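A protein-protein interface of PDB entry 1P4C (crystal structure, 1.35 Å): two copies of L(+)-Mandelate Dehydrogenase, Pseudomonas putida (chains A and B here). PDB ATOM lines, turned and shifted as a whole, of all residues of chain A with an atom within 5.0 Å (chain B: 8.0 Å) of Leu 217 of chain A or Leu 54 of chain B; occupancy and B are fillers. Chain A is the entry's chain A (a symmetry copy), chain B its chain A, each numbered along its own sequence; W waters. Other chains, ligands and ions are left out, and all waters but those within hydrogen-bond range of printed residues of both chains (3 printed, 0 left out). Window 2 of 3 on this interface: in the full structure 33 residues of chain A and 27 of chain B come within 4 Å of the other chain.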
ATOM      1  N   LEU A 155     -27.047 -27.698 -28.527  1.00  0.00           N
ATOM      2  CA  LEU A 155     -26.954 -28.159 -27.150  1.00  0.00           C
ATOM      3  C   LEU A 155     -27.583 -27.104 -26.251  1.00  0.00           C
ATOM      4  O   LEU A 155     -27.128 -25.965 -26.231  1.00  0.00           O
ATOM      5  CB  LEU A 155     -25.493 -28.354 -26.730  1.00  0.00           C
ATOM      6  CG  LEU A 155     -25.303 -28.659 -25.240  1.00  0.00           C
ATOM      7  CD1 LEU A 155     -25.850 -30.049 -24.935  1.00  0.00           C
ATOM      8  CD2 LEU A 155     -23.832 -28.564 -24.863  1.00  0.00           C
ATOM      9  N   THR A 157     -28.068 -25.599 -22.741  1.00  0.00           N
ATOM     10  CA  THR A 157     -27.327 -25.603 -21.490  1.00  0.00           C
ATOM     11  C   THR A 157     -27.963 -24.895 -20.303  1.00  0.00           C
ATOM     12  O   THR A 157     -27.356 -24.837 -19.231  1.00  0.00           O
ATOM     13  CB  THR A 157     -25.946 -24.954 -21.701  1.00  0.00           C
ATOM     14  OG1 THR A 157     -26.120 -23.563 -22.022  1.00  0.00           O
ATOM     15  CG2 THR A 157     -25.204 -25.635 -22.843  1.00  0.00           C
ATOM     16  N   PHE A 212     -22.507 -31.412 -16.809  1.00  0.00           N
ATOM     17  CA  PHE A 212     -22.068 -31.136 -18.173  1.00  0.00           C
ATOM     18  C   PHE A 212     -21.361 -29.787 -18.244  1.00  0.00           C
ATOM     19  O   PHE A 212     -21.977 -28.736 -18.064  1.00  0.00           O
ATOM     20  CB  PHE A 212     -23.259 -31.177 -19.133  1.00  0.00           C
ATOM     21  CG  PHE A 212     -22.876 -31.488 -20.554  1.00  0.00           C
ATOM     22  CD1 PHE A 212     -22.419 -30.489 -21.405  1.00  0.00           C
ATOM     23  CD2 PHE A 212     -22.947 -32.794 -21.031  1.00  0.00           C
ATOM     24  CE1 PHE A 212     -22.030 -30.785 -22.713  1.00  0.00           C
ATOM     25  CE2 PHE A 212     -22.561 -33.102 -22.335  1.00  0.00           C
ATOM     26  CZ  PHE A 212     -22.105 -32.094 -23.178  1.00  0.00           C
ATOM     27  N   ASN A 213     -20.057 -29.829 -18.505  1.00  0.00           N
ATOM     28  CA  ASN A 213     -19.244 -28.623 -18.568  1.00  0.00           C
ATOM     29  C   ASN A 213     -18.467 -28.464 -19.869  1.00  0.00           C
ATOM     30  O   ASN A 213     -18.734 -29.144 -20.856  1.00  0.00           O
ATOM     31  CB  ASN A 213     -18.262 -28.605 -17.398  1.00  0.00           C
ATOM     32  CG  ASN A 213     -17.425 -29.865 -17.325  1.00  0.00           C
ATOM     33  OD1 ASN A 213     -17.339 -30.624 -18.292  1.00  0.00           O
ATOM     34  ND2 ASN A 213     -16.791 -30.089 -16.180  1.00  0.00           N
ATOM     35  N   TRP A 214     -17.497 -27.555 -19.855  1.00  0.00           N
ATOM     36  CA  TRP A 214     -16.685 -27.287 -21.032  1.00  0.00           C
ATOM     37  C   TRP A 214     -15.991 -28.537 -21.555  1.00  0.00           C
ATOM     38  O   TRP A 214     -15.890 -28.732 -22.763  1.00  0.00           O
ATOM     39  CB  TRP A 214     -15.660 -26.194 -20.721  1.00  0.00           C
ATOM     40  CG  TRP A 214     -16.308 -24.889 -20.371  1.00  0.00           C
ATOM     41  CD1 TRP A 214     -16.335 -24.290 -19.145  1.00  0.00           C
ATOM     42  CD2 TRP A 214     -17.068 -24.049 -21.247  1.00  0.00           C
ATOM     43  NE1 TRP A 214     -17.069 -23.127 -19.203  1.00  0.00           N
ATOM     44  CE2 TRP A 214     -17.529 -22.956 -20.481  1.00  0.00           C
ATOM     45  CE3 TRP A 214     -17.406 -24.114 -22.605  1.00  0.00           C
ATOM     46  CZ2 TRP A 214     -18.313 -21.934 -21.028  1.00  0.00           C
ATOM     47  CZ3 TRP A 214     -18.187 -23.098 -23.149  1.00  0.00           C
ATOM     48  CH2 TRP A 214     -18.631 -22.022 -22.359  1.00  0.00           C
ATOM     49  N   GLU A 215     -15.522 -29.382 -20.644  1.00  0.00           N
ATOM     50  CA  GLU A 215     -14.854 -30.619 -21.034  1.00  0.00           C
ATOM     51  C   GLU A 215     -15.844 -31.506 -21.788  1.00  0.00           C
ATOM     52  O   GLU A 215     -15.502 -32.120 -22.801  1.00  0.00           O
ATOM     53  CB  GLU A 215     -14.333 -31.351 -19.794  1.00  0.00           C
ATOM     54  CG  GLU A 215     -13.604 -32.650 -20.101  1.00  0.00           C
ATOM     55  CD  GLU A 215     -13.139 -33.364 -18.851  1.00  0.00           C
ATOM     56  OE1 GLU A 215     -13.676 -33.070 -17.763  1.00  0.00           O
ATOM     57  OE2 GLU A 215     -12.246 -34.231 -18.956  1.00  0.00           O
ATOM     58  N   ALA A 216     -17.076 -31.562 -21.291  1.00  0.00           N
ATOM     59  CA  ALA A 216     -18.121 -32.364 -21.915  1.00  0.00           C
ATOM     60  C   ALA A 216     -18.494 -31.807 -23.285  1.00  0.00           C
ATOM     61  O   ALA A 216     -18.841 -32.561 -24.195  1.00  0.00           O
ATOM     62  CB  ALA A 216     -19.350 -32.412 -21.014  1.00  0.00           C
ATOM     63  N   LEU A 217     -18.433 -30.486 -23.431  1.00  0.00           N
ATOM     64  CA  LEU A 217     -18.747 -29.862 -24.711  1.00  0.00           C
ATOM     65  C   LEU A 217     -17.721 -30.320 -25.748  1.00  0.00           C
ATOM     66  O   LEU A 217     -18.059 -30.548 -26.905  1.00  0.00           O
ATOM     67  CB  LEU A 217     -18.727 -28.332 -24.592  1.00  0.00           C
ATOM     68  CG  LEU A 217     -18.946 -27.550 -25.895  1.00  0.00           C
ATOM     69  CD1 LEU A 217     -20.288 -27.921 -26.513  1.00  0.00           C
ATOM     70  CD2 LEU A 217     -18.884 -26.056 -25.615  1.00  0.00           C
ATOM     71  N   ARG A 218     -16.468 -30.456 -25.321  1.00  0.00           N
ATOM     72  CA  ARG A 218     -15.401 -30.903 -26.213  1.00  0.00           C
ATOM     73  C   ARG A 218     -15.731 -32.313 -26.695  1.00  0.00           C
ATOM     74  O   ARG A 218     -15.522 -32.653 -27.859  1.00  0.00           O
ATOM     75  CB  ARG A 218     -14.061 -30.901 -25.474  1.00  0.00           C
ATOM     76  CG  ARG A 218     -13.642 -29.528 -24.972  1.00  0.00           C
ATOM     77  CD  ARG A 218     -12.460 -29.618 -24.018  1.00  0.00           C
ATOM     78  NE  ARG A 218     -12.123 -28.316 -23.452  1.00  0.00           N
ATOM     79  CZ  ARG A 218     -11.542 -28.146 -22.270  1.00  0.00           C
ATOM     80  NH1 ARG A 218     -11.232 -29.201 -21.525  1.00  0.00           N
ATOM     81  NH2 ARG A 218     -11.271 -26.923 -21.833  1.00  0.00           N
ATOM     82  N   TRP A 219     -16.249 -33.126 -25.782  1.00  0.00           N
ATOM     83  CA  TRP A 219     -16.639 -34.494 -26.091  1.00  0.00           C
ATOM     84  C   TRP A 219     -17.720 -34.482 -27.173  1.00  0.00           C
ATOM     85  O   TRP A 219     -17.632 -35.203 -28.170  1.00  0.00           O
ATOM     86  CB  TRP A 219     -17.166 -35.170 -24.823  1.00  0.00           C
ATOM     87  CG  TRP A 219     -17.906 -36.446 -25.068  1.00  0.00           C
ATOM     88  CD1 TRP A 219     -17.374 -37.656 -25.414  1.00  0.00           C
ATOM     89  CD2 TRP A 219     -19.323 -36.633 -25.000  1.00  0.00           C
ATOM     90  NE1 TRP A 219     -18.376 -38.586 -25.565  1.00  0.00           N
ATOM     91  CE2 TRP A 219     -19.582 -37.985 -25.318  1.00  0.00           C
ATOM     92  CE3 TRP A 219     -20.402 -35.787 -24.703  1.00  0.00           C
ATOM     93  CZ2 TRP A 219     -20.878 -38.513 -25.347  1.00  0.00           C
ATOM     94  CZ3 TRP A 219     -21.689 -36.312 -24.731  1.00  0.00           C
ATOM     95  CH2 TRP A 219     -21.915 -37.664 -25.051  1.00  0.00           C
ATOM     96  N   LEU A 220     -18.738 -33.648 -26.978  1.00  0.00           N
ATOM     97  CA  LEU A 220     -19.830 -33.543 -27.937  1.00  0.00           C
ATOM     98  C   LEU A 220     -19.343 -33.018 -29.285  1.00  0.00           C
ATOM     99  O   LEU A 220     -19.804 -33.463 -30.338  1.00  0.00           O
ATOM    100  CB  LEU A 220     -20.924 -32.619 -27.394  1.00  0.00           C
ATOM    101  CG  LEU A 220     -22.162 -32.443 -28.278  1.00  0.00           C
ATOM    102  CD1 LEU A 220     -22.855 -33.784 -28.482  1.00  0.00           C
ATOM    103  CD2 LEU A 220     -23.111 -31.453 -27.621  1.00  0.00           C
ATOM    104  N   ARG A 221     -18.413 -32.068 -29.247  1.00  0.00           N
ATOM    105  CA  ARG A 221     -17.860 -31.473 -30.462  1.00  0.00           C
ATOM    106  C   ARG A 221     -17.191 -32.519 -31.349  1.00  0.00           C
ATOM    107  O   ARG A 221     -17.258 -32.434 -32.573  1.00  0.00           O
ATOM    108  CB  ARG A 221     -16.842 -30.385 -30.092  1.00  0.00           C
ATOM    109  CG  ARG A 221     -16.002 -29.841 -31.251  1.00  0.00           C
ATOM    110  CD  ARG A 221     -16.798 -28.981 -32.231  1.00  0.00           C
ATOM    111  NE  ARG A 221     -17.653 -29.763 -33.122  1.00  0.00           N
ATOM    112  CZ  ARG A 221     -18.391 -29.240 -34.096  1.00  0.00           C
ATOM    113  NH1 ARG A 221     -18.386 -27.929 -34.312  1.00  0.00           N
ATOM    114  NH2 ARG A 221     -19.136 -30.024 -34.862  1.00  0.00           N
ATOM    115  N   LEU A 228     -22.553 -27.114 -35.033  1.00  0.00           N
ATOM    116  CA  LEU A 228     -22.911 -27.260 -33.626  1.00  0.00           C
ATOM    117  C   LEU A 228     -23.113 -25.895 -32.977  1.00  0.00           C
ATOM    118  O   LEU A 228     -22.248 -25.024 -33.071  1.00  0.00           O
ATOM    119  CB  LEU A 228     -21.802 -28.010 -32.878  1.00  0.00           C
ATOM    120  CG  LEU A 228     -21.885 -28.091 -31.348  1.00  0.00           C
ATOM    121  CD1 LEU A 228     -23.101 -28.898 -30.920  1.00  0.00           C
ATOM    122  CD2 LEU A 228     -20.613 -28.728 -30.814  1.00  0.00           C
ATOM    123  N   VAL A 230     -24.458 -23.768 -29.334  1.00  0.00           N
ATOM    124  CA  VAL A 230     -24.706 -23.890 -27.907  1.00  0.00           C
ATOM    125  C   VAL A 230     -25.787 -22.866 -27.581  1.00  0.00           C
ATOM    126  O   VAL A 230     -25.629 -21.674 -27.847  1.00  0.00           O
ATOM    127  CB  VAL A 230     -23.437 -23.617 -27.089  1.00  0.00           C
ATOM    128  CG1 VAL A 230     -23.742 -23.733 -25.600  1.00  0.00           C
ATOM    129  CG2 VAL A 230     -22.345 -24.611 -27.489  1.00  0.00           C
ATOM    130  N   CYS A 242     -17.494 -20.702 -26.099  1.00  0.00           N
ATOM    131  CA  CYS A 242     -18.103 -21.757 -26.903  1.00  0.00           C
ATOM    132  C   CYS A 242     -17.428 -21.841 -28.265  1.00  0.00           C
ATOM    133  O   CYS A 242     -17.184 -22.934 -28.776  1.00  0.00           O
ATOM    134  CB  CYS A 242     -19.599 -21.504 -27.086  1.00  0.00           C
ATOM    135  SG  CYS A 242     -20.586 -21.888 -25.628  1.00  0.00           S
ATOM    136  N   GLU A 245     -14.105 -23.392 -27.957  1.00  0.00           N
ATOM    137  CA  GLU A 245     -14.205 -24.829 -27.710  1.00  0.00           C
ATOM    138  C   GLU A 245     -14.670 -25.623 -28.926  1.00  0.00           C
ATOM    139  O   GLU A 245     -14.814 -26.844 -28.848  1.00  0.00           O
ATOM    140  CB  GLU A 245     -15.143 -25.114 -26.531  1.00  0.00           C
ATOM    141  CG  GLU A 245     -14.665 -24.603 -25.176  1.00  0.00           C
ATOM    142  CD  GLU A 245     -13.354 -25.224 -24.723  1.00  0.00           C
ATOM    143  OE1 GLU A 245     -13.005 -26.322 -25.208  1.00  0.00           O
ATOM    144  OE2 GLU A 245     -12.678 -24.617 -23.866  1.00  0.00           O
ATOM    145  N   PRO B  51     -25.802 -15.616 -15.924  1.00  0.00           N
ATOM    146  CA  PRO B  51     -25.333 -16.967 -15.612  1.00  0.00           C
ATOM    147  C   PRO B  51     -24.063 -17.365 -16.340  1.00  0.00           C
ATOM    148  O   PRO B  51     -23.788 -16.893 -17.445  1.00  0.00           O
ATOM    149  CB  PRO B  51     -26.504 -17.847 -16.038  1.00  0.00           C
ATOM    150  CG  PRO B  51     -27.690 -16.971 -15.826  1.00  0.00           C
ATOM    151  CD  PRO B  51     -27.212 -15.636 -16.357  1.00  0.00           C
ATOM    152  N   LYS B  52     -23.292 -18.232 -15.699  1.00  0.00           N
ATOM    153  CA  LYS B  52     -22.078 -18.777 -16.287  1.00  0.00           C
ATOM    154  C   LYS B  52     -22.489 -20.197 -16.661  1.00  0.00           C
ATOM    155  O   LYS B  52     -22.798 -21.014 -15.789  1.00  0.00           O
ATOM    156  CB  LYS B  52     -20.936 -18.787 -15.269  1.00  0.00           C
ATOM    157  CG  LYS B  52     -20.503 -17.387 -14.849  1.00  0.00           C
ATOM    158  CD  LYS B  52     -19.261 -17.407 -13.972  1.00  0.00           C
ATOM    159  CE  LYS B  52     -18.913 -16.004 -13.488  1.00  0.00           C
ATOM    160  NZ  LYS B  52     -18.708 -15.061 -14.621  1.00  0.00           N
ATOM    161  N   ARG B  53     -22.533 -20.472 -17.961  1.00  0.00           N
ATOM    162  CA  ARG B  53     -22.943 -21.779 -18.460  1.00  0.00           C
ATOM    163  C   ARG B  53     -21.823 -22.803 -18.519  1.00  0.00           C
ATOM    164  O   ARG B  53     -20.643 -22.468 -18.430  1.00  0.00           O
ATOM    165  CB  ARG B  53     -23.560 -21.641 -19.855  1.00  0.00           C
ATOM    166  CG  ARG B  53     -24.859 -20.848 -19.893  1.00  0.00           C
ATOM    167  CD  ARG B  53     -25.970 -21.544 -19.131  1.00  0.00           C
ATOM    168  NE  ARG B  53     -27.167 -20.712 -19.068  1.00  0.00           N
ATOM    169  CZ  ARG B  53     -27.887 -20.527 -17.966  1.00  0.00           C
ATOM    170  NH1 ARG B  53     -27.540 -21.118 -16.833  1.00  0.00           N
ATOM    171  NH2 ARG B  53     -28.943 -19.728 -17.998  1.00  0.00           N
ATOM    172  N   LEU B  54     -22.223 -24.060 -18.676  1.00  0.00           N
ATOM    173  CA  LEU B  54     -21.300 -25.180 -18.772  1.00  0.00           C
ATOM    174  C   LEU B  54     -20.350 -25.296 -17.593  1.00  0.00           C
ATOM    175  O   LEU B  54     -19.168 -25.612 -17.745  1.00  0.00           O
ATOM    176  CB  LEU B  54     -20.542 -25.112 -20.099  1.00  0.00           C
ATOM    177  CG  LEU B  54     -21.498 -25.442 -21.251  1.00  0.00           C
ATOM    178  CD1 LEU B  54     -20.882 -25.078 -22.587  1.00  0.00           C
ATOM    179  CD2 LEU B  54     -21.853 -26.922 -21.206  1.00  0.00           C
ATOM    180  N   VAL B  55     -20.895 -25.022 -16.412  1.00  0.00           N
ATOM    181  CA  VAL B  55     -20.165 -25.145 -15.164  1.00  0.00           C
ATOM    182  C   VAL B  55     -20.782 -26.356 -14.476  1.00  0.00           C
ATOM    183  O   VAL B  55     -22.005 -26.519 -14.467  1.00  0.00           O
ATOM    184  CB  VAL B  55     -20.360 -23.916 -14.250  1.00  0.00           C
ATOM    185  CG1 VAL B  55     -19.741 -24.181 -12.880  1.00  0.00           C
ATOM    186  CG2 VAL B  55     -19.725 -22.692 -14.882  1.00  0.00           C
ATOM    187  N   ASP B  56     -19.939 -27.218 -13.924  1.00  0.00           N
ATOM    188  CA  ASP B  56     -20.422 -28.397 -13.223  1.00  0.00           C
ATOM    189  C   ASP B  56     -21.078 -27.948 -11.921  1.00  0.00           C
ATOM    190  O   ASP B  56     -20.397 -27.514 -10.995  1.00  0.00           O
ATOM    191  CB  ASP B  56     -19.246 -29.337 -12.934  1.00  0.00           C
ATOM    192  CG  ASP B  56     -19.654 -30.583 -12.169  1.00  0.00           C
ATOM    193  OD1 ASP B  56     -20.841 -30.726 -11.812  1.00  0.00           O
ATOM    194  OD2 ASP B  56     -18.770 -31.431 -11.917  1.00  0.00           O
ATOM    195  N   VAL B  57     -22.403 -28.035 -11.862  1.00  0.00           N
ATOM    196  CA  VAL B  57     -23.131 -27.646 -10.661  1.00  0.00           C
ATOM    197  C   VAL B  57     -23.859 -28.848 -10.068  1.00  0.00           C
ATOM    198  O   VAL B  57     -24.880 -28.701  -9.399  1.00  0.00           O
ATOM    199  CB  VAL B  57     -24.152 -26.510 -10.952  1.00  0.00           C
ATOM    200  CG1 VAL B  57     -23.412 -25.247 -11.368  1.00  0.00           C
ATOM    201  CG2 VAL B  57     -25.130 -26.932 -12.037  1.00  0.00           C
ATOM    202  N   ALA B 338     -27.363 -22.966  -8.898  1.00  0.00           N
ATOM    203  CA  ALA B 338     -27.219 -23.898 -10.006  1.00  0.00           C
ATOM    204  C   ALA B 338     -27.466 -23.175 -11.322  1.00  0.00           C
ATOM    205  O   ALA B 338     -26.703 -23.320 -12.278  1.00  0.00           O
ATOM    206  CB  ALA B 338     -28.204 -25.051  -9.854  1.00  0.00           C
ATOM    207  N   ILE B 340     -27.186 -19.962 -12.084  1.00  0.00           N
ATOM    208  CA  ILE B 340     -26.218 -18.945 -12.481  1.00  0.00           C
ATOM    209  C   ILE B 340     -24.803 -19.503 -12.614  1.00  0.00           C
ATOM    210  O   ILE B 340     -23.870 -18.776 -12.937  1.00  0.00           O
ATOM    211  CB  ILE B 340     -26.209 -17.726 -11.517  1.00  0.00           C
ATOM    212  CG1 ILE B 340     -25.703 -18.127 -10.132  1.00  0.00           C
ATOM    213  CG2 ILE B 340     -27.614 -17.131 -11.434  1.00  0.00           C
ATOM    214  CD1 ILE B 340     -25.570 -16.942  -9.179  1.00  0.00           C
ATOM    215  N   GLY B 341     -24.656 -20.801 -12.367  1.00  0.00           N
ATOM    216  CA  GLY B 341     -23.354 -21.431 -12.500  1.00  0.00           C
ATOM    217  C   GLY B 341     -22.347 -21.159 -11.402  1.00  0.00           C
ATOM    218  O   GLY B 341     -21.148 -21.080 -11.669  1.00  0.00           O
HETATM  219  O   HOH W   1     -24.788 -25.270 -18.266  1.00  0.00           O
HETATM  220  O   HOH W   2     -23.803 -27.413 -16.632  1.00  0.00           O
HETATM  221  O   HOH W   3     -17.173 -27.266 -14.324  1.00  0.00           O
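Of the 16 printed residues of chain A, 5 touch a printed residue of chain B.
Printed residues of chain A that touch a printed residue of chain B: Thr 157, Phe 212, Asn 213, Trp 214 and Leu 217.
Hydrophobic or aromatic side chains of chain A that line the printed part of chain B: Phe 212, Trp 214 and Leu 217.
Of the 10 printed residues of chain B, 2 touch a printed residue of chain A.
Among the printed residues, 7 pairs touch across the chains.
Among the printed residues, pairs that only touch across the chains: Asn 213 of chain A with Leu 54 of chain B (3.1 Å), Thr 157 of chain A with Arg 53 of chain B (3.5 Å), Trp 214 of chain A with Arg 53 of chain B (3.5 Å), Phe 212 of chain A with Leu 54 of chain B (3.6 Å), Leu 217 of chain A with Leu 54 of chain B (3.8 Å) and Thr 157 of chain A with Leu 54 of chain B (3.9 Å).
Water W2 lies within hydrogen-bond range of O of Phe 212 of chain A (2.7 Å) and O of Val 55 of chain B (3.0 Å).
Water W1 bridges O of Thr 157 of chain A (2.8 Å) and N of Leu 54 of chain B (2.9 Å).
Water W3 bridges the backbone NH (N) of Asp 56 of chain B and the side-chain amide nitrogen (ND2) of Asn 213 of chain A.
OD1 of Asn 213 of chain A lies close to N of Glu 215 of chain A (3.2 Å).
OD1 of Asn 213 of chain A lies within hydrogen-bond range of N of Ala 216 of chain A (3.2 Å).
The backbone carbonyl oxygen (O) of Leu 54 of chain B lies within hydrogen-bond range of the backbone NH (N) of Trp 214 of chain A (3.3 Å).
No position is printed for both chains.
Of the 7 pairs that touch across the chains among the printed residues, none has its exchanged pair printed and touching as well.
Printed residues of chain B within 4 Å of Asn 213 of chain A: Leu 54 (3.1 Å).
Of the printed residues of chain B, Trp 214 of chain A touches Arg 53 and Leu 54.
No residue of chain B comes within 4 Å of Ala 216 of chain A.
Leu 217 of chain A touches one residue of chain B.
Printed residues of chain A within 4 Å of Leu 54 of chain B: Thr 157 (3.9 Å), Phe 212 (3.6 Å), Asn 213 (3.1 Å), Trp 214 (3.3 Å) and Leu 217 (3.8 Å).
Val 55 of chain B touches none of the printed residues of chain A.
The nearest printed residue of chain B that does not touch Leu 217 of chain A is Arg 53 of chain B (8.2 Å).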
